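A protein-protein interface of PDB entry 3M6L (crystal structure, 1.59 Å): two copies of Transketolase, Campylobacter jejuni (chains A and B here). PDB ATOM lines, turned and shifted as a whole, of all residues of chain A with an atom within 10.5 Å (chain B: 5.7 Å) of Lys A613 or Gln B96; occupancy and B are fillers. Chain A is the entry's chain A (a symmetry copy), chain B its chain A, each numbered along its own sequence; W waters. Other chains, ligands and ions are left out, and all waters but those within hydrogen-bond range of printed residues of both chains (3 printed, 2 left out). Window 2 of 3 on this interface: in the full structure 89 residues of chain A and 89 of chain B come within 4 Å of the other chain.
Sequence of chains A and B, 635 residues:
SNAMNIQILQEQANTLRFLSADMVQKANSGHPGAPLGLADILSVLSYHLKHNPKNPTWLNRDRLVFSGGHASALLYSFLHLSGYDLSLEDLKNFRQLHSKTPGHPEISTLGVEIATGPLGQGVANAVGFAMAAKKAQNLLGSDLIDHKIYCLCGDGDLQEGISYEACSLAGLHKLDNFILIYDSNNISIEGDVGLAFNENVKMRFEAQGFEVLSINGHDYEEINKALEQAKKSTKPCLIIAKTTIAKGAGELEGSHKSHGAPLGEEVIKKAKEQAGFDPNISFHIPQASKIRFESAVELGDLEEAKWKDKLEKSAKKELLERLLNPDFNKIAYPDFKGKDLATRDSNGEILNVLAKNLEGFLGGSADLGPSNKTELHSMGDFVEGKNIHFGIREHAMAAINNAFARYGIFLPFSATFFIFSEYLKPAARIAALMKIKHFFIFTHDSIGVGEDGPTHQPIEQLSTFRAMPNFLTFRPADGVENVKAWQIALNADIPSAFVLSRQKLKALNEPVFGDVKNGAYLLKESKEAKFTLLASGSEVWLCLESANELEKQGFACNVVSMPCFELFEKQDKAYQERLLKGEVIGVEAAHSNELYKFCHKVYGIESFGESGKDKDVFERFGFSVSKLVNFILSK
Of the 25 printed residues of chain A, 7 touch a printed residue of chain B.
Printed residues of chain A that touch a printed residue of chain B: Glu A451, Asp A452, Glu A610, Ser A611, Gly A612, Lys A613 and Asp A616.
Of the 12 printed residues of chain B, 4 touch a printed residue of chain A.
Hydrophobic or aromatic side chains of chain B that line the printed part of chain A: Leu B97.
Among the printed residues, Asp or Glu carboxylates within 4 Å of a Lys or Arg side-chain nitrogen of the other chain: Asp A452 with Arg B95 (3.0 Å).
No position is printed for both chains.
Arg B95 touches Glu A451 (NH1 to CB, 3.3 Å).
Glu A610 touches Leu B97 (CB to CD1, 3.8 Å).
OG of Ser A611 touches CA of Arg B95, 3.7 Å away.
Arg B95 touches Gly A612.
Gly A612 touches Leu B97 (CA to N, 3.7 Å).
O of Ala B27 touches NZ of Lys A613, at 3.8 Å.
Lys A613 touches Gln B96.
CD2 of Leu B97 touches O of Asp A616 (3.8 Å).
Of the printed residues of chain B, Glu A451 touches Arg B95.
Of the printed residues of chain B, Asp A452 touches Arg B95.
Of the printed residues of chain B, Ser A611 touches Arg B95 (3.7 Å), Gln B96 (3.4 Å) and Leu B97 (3.4 Å).
Of chain B, only Ala B27 (3.8 Å) and Gln B96 (3.5 Å) come within 4 Å of Lys A613.
Of the printed residues of chain B, Asp A616 touches Leu B97.
Of the printed residues of chain A, Ala B27 touches Lys A613 (3.8 Å).
No residue of chain A comes within 4 Å of Asn B93.
Of the printed residues of chain A, Arg B95 touches Glu A451, Asp A452, Ser A611 and Gly A612.
Leu B97 touches four residues of chain A.
No residue of chain A comes within 4 Å of Ser B99.
The nearest residue of chain A that does not touch Gln B96 is Gly A612 (4.1 Å).
The nearest printed residue of chain B that does not touch Glu A451 is Ala B27 (4.5 Å).
OG of Ser A611 sits at hydrogen-bond distance from O of Glu A451, at 2.7 Å.
The backbone carbonyl oxygen of Gln B96 is in hydrogen-bond range of the side-chain hydroxyl of Ser B99 (3.3 Å).
The backbone carbonyl oxygen (O) of Thr B101 sits at hydrogen-bond distance from the backbone NH (N) of Arg B95, at 2.9 Å.
NE2 of Gln A457 sits at hydrogen-bond distance from O of Glu A610 (2.9 Å).
OE1 of Gln B96 sits close to O of Phe B94, 3.0 Å away.
NH2 of Arg B95 lies within salt-bridge range of OD1 of Asp A452 (3.0 Å).
O of Gln B96 lies close to O of Ser A611 (3.4 Å).
The backbone NH of Leu B97 sits close to the backbone carbonyl oxygen of Ser A611 (3.4 Å).
Water W1 lies within hydrogen-bond range of the backbone NH of His B98 (2.8 Å), the side-chain carboxylate of Glu A610 (2.8 Å) and the backbone carbonyl oxygen of Ser A611 (2.9 Å).
Water W2 lies within hydrogen-bond range of O of Gln B96 (2.8 Å), OG of Ser B99 (2.9 Å) and O of Ser A611 (3.3 Å).
Water W3 lies within hydrogen-bond range of NZ of Lys A613 (2.9 Å) and O of Lys B26 (3.1 Å).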
ATOM      1  N   SER A 446       4.219  -2.557 -22.572  1.00  0.00           N
ATOM      2  CA  SER A 446       4.428  -1.618 -21.453  1.00  0.00           C
ATOM      3  C   SER A 446       5.597  -1.975 -20.636  1.00  0.00           C
ATOM      4  O   SER A 446       6.317  -2.906 -20.970  1.00  0.00           O
ATOM      5  CB  SER A 446       3.172  -1.600 -20.564  1.00  0.00           C
ATOM      6  OG  SER A 446       3.203  -2.706 -19.695  1.00  0.00           O
ATOM      7  N   ILE A 447       5.880  -1.160 -19.622  1.00  0.00           N
ATOM      8  CA  ILE A 447       6.793  -1.561 -18.553  1.00  0.00           C
ATOM      9  C   ILE A 447       6.612  -2.980 -17.982  1.00  0.00           C
ATOM     10  O   ILE A 447       7.558  -3.516 -17.493  1.00  0.00           O
ATOM     11  CB  ILE A 447       6.804  -0.465 -17.405  1.00  0.00           C
ATOM     12  CG1 ILE A 447       5.408  -0.164 -16.932  1.00  0.00           C
ATOM     13  CG2 ILE A 447       7.548   0.765 -17.854  1.00  0.00           C
ATOM     14  CD1 ILE A 447       5.436   0.503 -15.538  1.00  0.00           C
ATOM     15  N   GLY A 448       5.425  -3.563 -18.194  1.00  0.00           N
ATOM     16  CA  GLY A 448       5.147  -4.958 -17.870  1.00  0.00           C
ATOM     17  C   GLY A 448       6.078  -5.964 -18.518  1.00  0.00           C
ATOM     18  O   GLY A 448       6.172  -7.105 -18.079  1.00  0.00           O
ATOM     19  N   VAL A 449       6.740  -5.555 -19.589  1.00  0.00           N
ATOM     20  CA  VAL A 449       7.888  -6.290 -20.189  1.00  0.00           C
ATOM     21  C   VAL A 449       8.933  -6.703 -19.142  1.00  0.00           C
ATOM     22  O   VAL A 449       9.432  -7.827 -19.162  1.00  0.00           O
ATOM     23  CB  VAL A 449       8.503  -5.416 -21.315  1.00  0.00           C
ATOM     24  CG1 VAL A 449       9.994  -5.856 -21.655  1.00  0.00           C
ATOM     25  CG2 VAL A 449       7.544  -5.371 -22.601  1.00  0.00           C
ATOM     26  N   GLY A 450       9.225  -5.837 -18.165  1.00  0.00           N
ATOM     27  CA  GLY A 450      10.081  -6.242 -17.098  1.00  0.00           C
ATOM     28  C   GLY A 450      11.555  -6.139 -17.409  1.00  0.00           C
ATOM     29  O   GLY A 450      12.174  -5.069 -17.636  1.00  0.00           O
ATOM     30  N   GLU A 451      12.225  -7.262 -17.358  1.00  0.00           N
ATOM     31  CA  GLU A 451      13.654  -7.319 -17.310  1.00  0.00           C
ATOM     32  C   GLU A 451      14.430  -6.774 -18.521  1.00  0.00           C
ATOM     33  O   GLU A 451      15.571  -6.320 -18.375  1.00  0.00           O
ATOM     34  CB  GLU A 451      14.129  -8.771 -17.081  1.00  0.00           C
ATOM     35  CG  GLU A 451      13.872  -9.298 -15.630  1.00  0.00           C
ATOM     36  CD  GLU A 451      12.490  -9.975 -15.486  1.00  0.00           C
ATOM     37  OE1 GLU A 451      11.571  -9.768 -16.285  1.00  0.00           O
ATOM     38  OE2 GLU A 451      12.362 -10.779 -14.519  1.00  0.00           O
ATOM     39  N   ASP A 452      13.841  -6.856 -19.706  1.00  0.00           N
ATOM     40  CA  ASP A 452      14.561  -6.324 -20.859  1.00  0.00           C
ATOM     41  C   ASP A 452      14.845  -4.816 -20.721  1.00  0.00           C
ATOM     42  O   ASP A 452      15.759  -4.328 -21.335  1.00  0.00           O
ATOM     43  CB  ASP A 452      13.835  -6.577 -22.185  1.00  0.00           C
ATOM     44  CG  ASP A 452      13.966  -8.064 -22.677  1.00  0.00           C
ATOM     45  OD1 ASP A 452      14.915  -8.767 -22.264  1.00  0.00           O
ATOM     46  OD2 ASP A 452      13.164  -8.497 -23.544  1.00  0.00           O
ATOM     47  N   GLY A 453      14.071  -4.110 -19.898  1.00  0.00           N
ATOM     48  CA  GLY A 453      14.401  -2.752 -19.579  1.00  0.00           C
ATOM     49  C   GLY A 453      13.941  -1.697 -20.557  1.00  0.00           C
ATOM     50  O   GLY A 453      13.184  -1.940 -21.451  1.00  0.00           O
ATOM     51  N   PRO A 454      14.504  -0.498 -20.362  1.00  0.00           N
ATOM     52  CA  PRO A 454      13.813   0.646 -20.988  1.00  0.00           C
ATOM     53  C   PRO A 454      13.878   0.776 -22.484  1.00  0.00           C
ATOM     54  O   PRO A 454      12.999   1.413 -23.056  1.00  0.00           O
ATOM     55  CB  PRO A 454      14.482   1.887 -20.291  1.00  0.00           C
ATOM     56  CG  PRO A 454      15.682   1.453 -19.644  1.00  0.00           C
ATOM     57  CD  PRO A 454      15.432  -0.071 -19.324  1.00  0.00           C
ATOM     58  N   GLN A 457      10.678  -1.039 -23.379  1.00  0.00           N
ATOM     59  CA  GLN A 457       9.424  -0.723 -22.680  1.00  0.00           C
ATOM     60  C   GLN A 457       8.846   0.467 -23.349  1.00  0.00           C
ATOM     61  O   GLN A 457       9.350   1.612 -23.233  1.00  0.00           O
ATOM     62  CB  GLN A 457       9.687  -0.528 -21.136  1.00  0.00           C
ATOM     63  CG  GLN A 457      10.082  -1.810 -20.421  1.00  0.00           C
ATOM     64  CD  GLN A 457      10.697  -1.564 -19.092  1.00  0.00           C
ATOM     65  OE1 GLN A 457      10.929  -0.410 -18.732  1.00  0.00           O
ATOM     66  NE2 GLN A 457      10.964  -2.608 -18.306  1.00  0.00           N
ATOM     67  N   ARG A 502       2.429  -8.742 -22.794  1.00  0.00           N
ATOM     68  CA  ARG A 502       3.275  -9.924 -22.546  1.00  0.00           C
ATOM     69  C   ARG A 502       2.664 -10.754 -21.446  1.00  0.00           C
ATOM     70  O   ARG A 502       2.667 -11.960 -21.488  1.00  0.00           O
ATOM     71  CB  ARG A 502       4.678  -9.482 -22.134  1.00  0.00           C
ATOM     72  CG  ARG A 502       5.687 -10.594 -21.976  1.00  0.00           C
ATOM     73  CD  ARG A 502       7.114 -10.107 -21.558  1.00  0.00           C
ATOM     74  NE  ARG A 502       8.071 -11.209 -21.541  1.00  0.00           N
ATOM     75  CZ  ARG A 502       8.589 -11.755 -20.443  1.00  0.00           C
ATOM     76  NH1 ARG A 502       9.456 -12.772 -20.572  1.00  0.00           N
ATOM     77  NH2 ARG A 502       8.283 -11.288 -19.211  1.00  0.00           N
ATOM     78  N   GLN A 503       2.224 -10.073 -20.393  1.00  0.00           N
ATOM     79  CA  GLN A 503       1.837 -10.666 -19.154  1.00  0.00           C
ATOM     80  C   GLN A 503       0.355 -10.989 -19.071  1.00  0.00           C
ATOM     81  O   GLN A 503      -0.483 -10.357 -19.728  1.00  0.00           O
ATOM     82  CB  GLN A 503       2.276  -9.746 -17.958  1.00  0.00           C
ATOM     83  CG  GLN A 503       1.364  -8.614 -17.627  1.00  0.00           C
ATOM     84  CD  GLN A 503       1.610  -7.369 -18.556  1.00  0.00           C
ATOM     85  OE1 GLN A 503       2.384  -7.446 -19.531  1.00  0.00           O
ATOM     86  NE2 GLN A 503       1.051  -6.226 -18.147  1.00  0.00           N
ATOM     87  N   GLY A 609      11.431   3.656 -18.675  1.00  0.00           N
ATOM     88  CA  GLY A 609      11.224   2.528 -17.757  1.00  0.00           C
ATOM     89  C   GLY A 609      12.472   2.101 -16.984  1.00  0.00           C
ATOM     90  O   GLY A 609      13.467   2.808 -16.927  1.00  0.00           O
ATOM     91  N   GLU A 610      12.456   0.868 -16.497  1.00  0.00           N
ATOM     92  CA  GLU A 610      13.544   0.299 -15.695  1.00  0.00           C
ATOM     93  C   GLU A 610      13.608  -1.194 -15.946  1.00  0.00           C
ATOM     94  O   GLU A 610      12.618  -1.849 -16.111  1.00  0.00           O
ATOM     95  CB  GLU A 610      13.254   0.475 -14.210  1.00  0.00           C
ATOM     96  CG  GLU A 610      13.333   1.862 -13.652  1.00  0.00           C
ATOM     97  CD  GLU A 610      14.727   2.420 -13.624  1.00  0.00           C
ATOM     98  OE1 GLU A 610      15.712   1.654 -13.654  1.00  0.00           O
ATOM     99  OE2 GLU A 610      14.837   3.662 -13.571  1.00  0.00           O
ATOM    100  N   SER A 611      14.821  -1.726 -15.909  1.00  0.00           N
ATOM    101  CA  SER A 611      15.024  -3.197 -15.976  1.00  0.00           C
ATOM    102  C   SER A 611      14.796  -3.825 -14.595  1.00  0.00           C
ATOM    103  O   SER A 611      15.497  -3.508 -13.628  1.00  0.00           O
ATOM    104  CB  SER A 611      16.482  -3.522 -16.458  1.00  0.00           C
ATOM    105  OG  SER A 611      16.792  -4.901 -16.449  1.00  0.00           O
ATOM    106  N   GLY A 612      13.800  -4.698 -14.545  1.00  0.00           N
ATOM    107  CA  GLY A 612      13.502  -5.385 -13.305  1.00  0.00           C
ATOM    108  C   GLY A 612      12.365  -6.376 -13.529  1.00  0.00           C
ATOM    109  O   GLY A 612      11.639  -6.404 -14.527  1.00  0.00           O
ATOM    110  N   LYS A 613      12.085  -7.173 -12.505  1.00  0.00           N
ATOM    111  CA  LYS A 613      10.882  -7.986 -12.550  1.00  0.00           C
ATOM    112  C   LYS A 613       9.631  -7.152 -12.735  1.00  0.00           C
ATOM    113  O   LYS A 613       9.514  -6.069 -12.138  1.00  0.00           O
ATOM    114  CB  LYS A 613      10.799  -8.785 -11.258  1.00  0.00           C
ATOM    115  CG  LYS A 613      11.937  -9.830 -11.089  1.00  0.00           C
ATOM    116  CD  LYS A 613      11.637 -10.727  -9.877  1.00  0.00           C
ATOM    117  CE  LYS A 613      12.790 -11.623  -9.489  1.00  0.00           C
ATOM    118  NZ  LYS A 613      13.189 -12.683 -10.510  1.00  0.00           N
ATOM    119  N   ASP A 614       8.721  -7.579 -13.582  1.00  0.00           N
ATOM    120  CA  ASP A 614       7.478  -6.885 -13.863  1.00  0.00           C
ATOM    121  C   ASP A 614       6.798  -6.342 -12.625  1.00  0.00           C
ATOM    122  O   ASP A 614       6.452  -5.176 -12.571  1.00  0.00           O
ATOM    123  CB  ASP A 614       6.488  -7.687 -14.755  1.00  0.00           C
ATOM    124  CG  ASP A 614       6.047  -9.044 -14.156  1.00  0.00           C
ATOM    125  OD1 ASP A 614       6.483  -9.456 -13.047  1.00  0.00           O
ATOM    126  OD2 ASP A 614       5.217  -9.689 -14.853  1.00  0.00           O
ATOM    127  N   LYS A 615       6.571  -7.193 -11.646  1.00  0.00           N
ATOM    128  CA  LYS A 615       5.932  -6.671 -10.388  1.00  0.00           C
ATOM    129  C   LYS A 615       6.750  -5.534  -9.729  1.00  0.00           C
ATOM    130  O   LYS A 615       6.100  -4.557  -9.266  1.00  0.00           O
ATOM    131  CB  LYS A 615       5.719  -7.804  -9.401  1.00  0.00           C
ATOM    132  CG  LYS A 615       4.644  -8.775  -9.875  1.00  0.00           C
ATOM    133  CD  LYS A 615       4.698 -10.091  -9.001  1.00  0.00           C
ATOM    134  CE  LYS A 615       3.672 -11.161  -9.424  1.00  0.00           C
ATOM    135  NZ  LYS A 615       2.381 -10.437  -9.777  1.00  0.00           N
ATOM    136  N   ASP A 616       8.090  -5.642  -9.693  1.00  0.00           N
ATOM    137  CA  ASP A 616       8.972  -4.643  -9.085  1.00  0.00           C
ATOM    138  C   ASP A 616       8.870  -3.325  -9.872  1.00  0.00           C
ATOM    139  O   ASP A 616       8.789  -2.197  -9.286  1.00  0.00           O
ATOM    140  CB  ASP A 616      10.428  -5.115  -9.039  1.00  0.00           C
ATOM    141  CG  ASP A 616      10.625  -6.269  -8.077  1.00  0.00           C
ATOM    142  OD1 ASP A 616       9.650  -6.497  -7.279  1.00  0.00           O
ATOM    143  OD2 ASP A 616      11.723  -6.854  -8.099  1.00  0.00           O
ATOM    144  N   VAL A 617       8.773  -3.430 -11.228  1.00  0.00           N
ATOM    145  CA  VAL A 617       8.731  -2.213 -12.101  1.00  0.00           C
ATOM    146  C   VAL A 617       7.368  -1.520 -12.005  1.00  0.00           C
ATOM    147  O   VAL A 617       7.263  -0.326 -11.830  1.00  0.00           O
ATOM    148  CB  VAL A 617       9.054  -2.560 -13.556  1.00  0.00           C
ATOM    149  CG1 VAL A 617       8.983  -1.223 -14.451  1.00  0.00           C
ATOM    150  CG2 VAL A 617      10.403  -3.135 -13.622  1.00  0.00           C
ATOM    151  N   PHE A 618       6.277  -2.267 -12.066  1.00  0.00           N
ATOM    152  CA  PHE A 618       4.983  -1.616 -11.866  1.00  0.00           C
ATOM    153  C   PHE A 618       4.878  -0.916 -10.500  1.00  0.00           C
ATOM    154  O   PHE A 618       4.279   0.176 -10.430  1.00  0.00           O
ATOM    155  CB  PHE A 618       3.835  -2.659 -11.968  1.00  0.00           C
ATOM    156  CG  PHE A 618       3.368  -2.924 -13.387  1.00  0.00           C
ATOM    157  CD1 PHE A 618       2.856  -1.895 -14.215  1.00  0.00           C
ATOM    158  CD2 PHE A 618       3.480  -4.203 -13.910  1.00  0.00           C
ATOM    159  CE1 PHE A 618       2.372  -2.142 -15.549  1.00  0.00           C
ATOM    160  CE2 PHE A 618       3.011  -4.486 -15.231  1.00  0.00           C
ATOM    161  CZ  PHE A 618       2.486  -3.464 -16.025  1.00  0.00           C
ATOM    162  N   GLU A 619       5.386  -1.541  -9.431  1.00  0.00           N
ATOM    163  CA  GLU A 619       5.392  -0.906  -8.075  1.00  0.00           C
ATOM    164  C   GLU A 619       6.229   0.398  -8.105  1.00  0.00           C
ATOM    165  O   GLU A 619       5.760   1.424  -7.624  1.00  0.00           O
ATOM    166  CB  GLU A 619       5.890  -1.914  -7.025  1.00  0.00           C
ATOM    167  CG  GLU A 619       5.772  -1.432  -5.573  1.00  0.00           C
ATOM    168  CD  GLU A 619       4.296  -1.160  -5.148  1.00  0.00           C
ATOM    169  OE1 GLU A 619       3.352  -1.941  -5.479  1.00  0.00           O
ATOM    170  OE2 GLU A 619       4.070  -0.120  -4.474  1.00  0.00           O
ATOM    171  N   ARG A 620       7.393   0.370  -8.737  1.00  0.00           N
ATOM    172  CA  ARG A 620       8.207   1.554  -8.819  1.00  0.00           C
ATOM    173  C   ARG A 620       7.474   2.713  -9.438  1.00  0.00           C
ATOM    174  O   ARG A 620       7.618   3.822  -9.006  1.00  0.00           O
ATOM    175  CB  ARG A 620       9.528   1.268  -9.555  1.00  0.00           C
ATOM    176  CG  ARG A 620      10.069   2.447 -10.347  1.00  0.00           C
ATOM    177  CD  ARG A 620      10.881   3.399  -9.531  1.00  0.00           C
ATOM    178  NE  ARG A 620      11.451   4.435 -10.404  1.00  0.00           N
ATOM    179  CZ  ARG A 620      10.830   5.514 -10.830  1.00  0.00           C
ATOM    180  NH1 ARG A 620       9.611   5.825 -10.465  1.00  0.00           N
ATOM    181  NH2 ARG A 620      11.450   6.301 -11.627  1.00  0.00           N
ATOM    182  N   PHE A 621       6.711   2.406 -10.483  1.00  0.00           N
ATOM    183  CA  PHE A 621       6.011   3.421 -11.261  1.00  0.00           C
ATOM    184  C   PHE A 621       4.619   3.759 -10.762  1.00  0.00           C
ATOM    185  O   PHE A 621       3.897   4.582 -11.288  1.00  0.00           O
ATOM    186  CB  PHE A 621       6.024   3.091 -12.774  1.00  0.00           C
ATOM    187  CG  PHE A 621       7.355   3.313 -13.411  1.00  0.00           C
ATOM    188  CD1 PHE A 621       7.791   4.612 -13.632  1.00  0.00           C
ATOM    189  CD2 PHE A 621       8.227   2.298 -13.634  1.00  0.00           C
ATOM    190  CE1 PHE A 621       9.052   4.828 -14.081  1.00  0.00           C
ATOM    191  CE2 PHE A 621       9.454   2.515 -14.138  1.00  0.00           C
ATOM    192  CZ  PHE A 621       9.860   3.789 -14.386  1.00  0.00           C
ATOM    193  N   LYS B  26      20.307 -17.040 -12.408  1.00  0.00           N
ATOM    194  CA  LYS B  26      19.954 -16.450 -11.121  1.00  0.00           C
ATOM    195  C   LYS B  26      18.821 -15.459 -11.328  1.00  0.00           C
ATOM    196  O   LYS B  26      17.851 -15.391 -10.565  1.00  0.00           O
ATOM    197  CB  LYS B  26      21.196 -15.820 -10.459  1.00  0.00           C
ATOM    198  CG  LYS B  26      20.877 -15.186  -9.064  1.00  0.00           C
ATOM    199  CD  LYS B  26      22.142 -14.823  -8.323  1.00  0.00           C
ATOM    200  CE  LYS B  26      21.864 -14.448  -6.874  1.00  0.00           C
ATOM    201  NZ  LYS B  26      21.007 -13.252  -6.855  1.00  0.00           N
ATOM    202  N   ALA B  27      18.913 -14.662 -12.401  1.00  0.00           N
ATOM    203  CA  ALA B  27      17.790 -13.803 -12.785  1.00  0.00           C
ATOM    204  C   ALA B  27      16.523 -14.484 -13.277  1.00  0.00           C
ATOM    205  O   ALA B  27      15.409 -13.887 -13.379  1.00  0.00           O
ATOM    206  CB  ALA B  27      18.245 -12.720 -13.859  1.00  0.00           C
ATOM    207  N   ASN B  28      16.657 -15.770 -13.678  1.00  0.00           N
ATOM    208  CA  ASN B  28      15.614 -16.452 -14.432  1.00  0.00           C
ATOM    209  C   ASN B  28      15.121 -15.665 -15.643  1.00  0.00           C
ATOM    210  O   ASN B  28      13.930 -15.630 -15.962  1.00  0.00           O
ATOM    211  CB  ASN B  28      14.419 -16.815 -13.578  1.00  0.00           C
ATOM    212  CG  ASN B  28      13.640 -18.002 -14.137  1.00  0.00           C
ATOM    213  OD1 ASN B  28      14.162 -18.810 -14.963  1.00  0.00           O
ATOM    214  ND2 ASN B  28      12.387 -18.138 -13.654  1.00  0.00           N
ATOM    215  N   LYS B  92      25.473 -10.647  -9.683  1.00  0.00           N
ATOM    216  CA  LYS B  92      24.415 -11.401  -9.090  1.00  0.00           C
ATOM    217  C   LYS B  92      23.087 -10.644  -9.014  1.00  0.00           C
ATOM    218  O   LYS B  92      22.068 -11.231  -8.659  1.00  0.00           O
ATOM    219  CB  LYS B  92      24.842 -11.848  -7.672  1.00  0.00           C
ATOM    220  CG  LYS B  92      26.099 -12.698  -7.677  1.00  0.00           C
ATOM    221  CD  LYS B  92      26.493 -13.082  -6.243  1.00  0.00           C
ATOM    222  CE  LYS B  92      27.788 -13.957  -6.237  1.00  0.00           C
ATOM    223  NZ  LYS B  92      28.210 -14.351  -4.808  1.00  0.00           N
ATOM    224  N   ASN B  93      23.089  -9.344  -9.357  1.00  0.00           N
ATOM    225  CA  ASN B  93      21.891  -8.585  -9.446  1.00  0.00           C
ATOM    226  C   ASN B  93      21.441  -8.268 -10.899  1.00  0.00           C
ATOM    227  O   ASN B  93      20.564  -7.429 -11.088  1.00  0.00           O
ATOM    228  CB  ASN B  93      21.977  -7.380  -8.591  1.00  0.00           C
ATOM    229  CG  ASN B  93      21.854  -7.853  -7.091  1.00  0.00           C
ATOM    230  OD1 ASN B  93      22.827  -8.006  -6.405  1.00  0.00           O
ATOM    231  ND2 ASN B  93      20.619  -8.186  -6.686  1.00  0.00           N
ATOM    232  N   PHE B  94      21.960  -9.063 -11.847  1.00  0.00           N
ATOM    233  CA  PHE B  94      21.519  -8.947 -13.233  1.00  0.00           C
ATOM    234  C   PHE B  94      20.019  -8.899 -13.364  1.00  0.00           C
ATOM    235  O   PHE B  94      19.265  -9.701 -12.783  1.00  0.00           O
ATOM    236  CB  PHE B  94      22.119 -10.142 -13.994  1.00  0.00           C
ATOM    237  CG  PHE B  94      21.847 -10.154 -15.486  1.00  0.00           C
ATOM    238  CD1 PHE B  94      22.371  -9.132 -16.283  1.00  0.00           C
ATOM    239  CD2 PHE B  94      21.243 -11.290 -16.076  1.00  0.00           C
ATOM    240  CE1 PHE B  94      22.202  -9.211 -17.710  1.00  0.00           C
ATOM    241  CE2 PHE B  94      21.088 -11.404 -17.483  1.00  0.00           C
ATOM    242  CZ  PHE B  94      21.589 -10.351 -18.280  1.00  0.00           C
ATOM    243  N   ARG B  95      19.551  -7.919 -14.150  1.00  0.00           N
ATOM    244  CA  ARG B  95      18.200  -7.720 -14.554  1.00  0.00           C
ATOM    245  C   ARG B  95      17.234  -7.377 -13.416  1.00  0.00           C
ATOM    246  O   ARG B  95      16.036  -7.440 -13.599  1.00  0.00           O
ATOM    247  CB  ARG B  95      17.710  -8.928 -15.374  1.00  0.00           C
ATOM    248  CG  ARG B  95      18.167  -8.913 -16.800  1.00  0.00           C
ATOM    249  CD  ARG B  95      17.901 -10.211 -17.608  1.00  0.00           C
ATOM    250  NE  ARG B  95      18.148  -9.861 -18.996  1.00  0.00           N
ATOM    251  CZ  ARG B  95      17.212  -9.578 -19.901  1.00  0.00           C
ATOM    252  NH1 ARG B  95      15.917  -9.854 -19.674  1.00  0.00           N
ATOM    253  NH2 ARG B  95      17.607  -8.991 -21.075  1.00  0.00           N
ATOM    254  N   GLN B  96      17.806  -7.027 -12.245  1.00  0.00           N
ATOM    255  CA  GLN B  96      16.992  -6.608 -11.088  1.00  0.00           C
ATOM    256  C   GLN B  96      16.862  -5.080 -10.962  1.00  0.00           C
ATOM    257  O   GLN B  96      17.760  -4.322 -11.267  1.00  0.00           O
ATOM    258  CB  GLN B  96      17.562  -7.147  -9.796  1.00  0.00           C
ATOM    259  CG  GLN B  96      17.694  -8.663  -9.858  1.00  0.00           C
ATOM    260  CD  GLN B  96      16.513  -9.338 -10.416  1.00  0.00           C
ATOM    261  OE1 GLN B  96      16.614 -10.017 -11.508  1.00  0.00           O
ATOM    262  NE2 GLN B  96      15.380  -9.260  -9.720  1.00  0.00           N
ATOM    263  N   LEU B  97      15.732  -4.677 -10.433  1.00  0.00           N
ATOM    264  CA  LEU B  97      15.420  -3.281 -10.261  1.00  0.00           C
ATOM    265  C   LEU B  97      16.525  -2.539  -9.539  1.00  0.00           C
ATOM    266  O   LEU B  97      16.955  -2.959  -8.444  1.00  0.00           O
ATOM    267  CB  LEU B  97      14.132  -3.106  -9.516  1.00  0.00           C
ATOM    268  CG  LEU B  97      13.627  -1.664  -9.472  1.00  0.00           C
ATOM    269  CD1 LEU B  97      13.150  -1.248 -10.843  1.00  0.00           C
ATOM    270  CD2 LEU B  97      12.433  -1.445  -8.477  1.00  0.00           C
ATOM    271  N   HIS B  98      16.987  -1.435 -10.159  1.00  0.00           N
ATOM    272  CA  HIS B  98      18.053  -0.576  -9.654  1.00  0.00           C
ATOM    273  C   HIS B  98      19.476  -1.099  -9.630  1.00  0.00           C
ATOM    274  O   HIS B  98      20.402  -0.446  -9.068  1.00  0.00           O
ATOM    275  CB  HIS B  98      17.683   0.007  -8.322  1.00  0.00           C
ATOM    276  CG  HIS B  98      16.409   0.818  -8.402  1.00  0.00           C
ATOM    277  ND1 HIS B  98      15.362   0.676  -7.505  1.00  0.00           N
ATOM    278  CD2 HIS B  98      15.978   1.700  -9.349  1.00  0.00           C
ATOM    279  CE1 HIS B  98      14.392   1.518  -7.838  1.00  0.00           C
ATOM    280  NE2 HIS B  98      14.724   2.129  -8.962  1.00  0.00           N
ATOM    281  N   SER B  99      19.681  -2.241 -10.271  1.00  0.00           N
ATOM    282  CA  SER B  99      21.047  -2.764 -10.366  1.00  0.00           C
ATOM    283  C   SER B  99      21.858  -2.042 -11.376  1.00  0.00           C
ATOM    284  O   SER B  99      21.307  -1.397 -12.311  1.00  0.00           O
ATOM    285  CB  SER B  99      21.068  -4.227 -10.647  1.00  0.00           C
ATOM    286  OG  SER B  99      20.955  -4.545 -12.005  1.00  0.00           O
ATOM    287  N   THR B 101      23.475  -3.717 -13.509  1.00  0.00           N
ATOM    288  CA  THR B 101      23.541  -4.694 -14.605  1.00  0.00           C
ATOM    289  C   THR B 101      22.149  -4.931 -15.256  1.00  0.00           C
ATOM    290  O   THR B 101      21.547  -6.059 -15.161  1.00  0.00           O
ATOM    291  CB  THR B 101      24.138  -6.044 -14.026  1.00  0.00           C
ATOM    292  OG1 THR B 101      23.502  -6.298 -12.751  1.00  0.00           O
ATOM    293  CG2 THR B 101      25.645  -5.917 -13.811  1.00  0.00           C
HETATM  294  O   HOH W   1      16.403  -0.931 -12.815  1.00  0.00           O
HETATM  295  O   HOH W   2      18.783  -3.618 -13.744  1.00  0.00           O
HETATM  296  O   HOH W   3      15.723 -13.481  -9.331  1.00  0.00           O
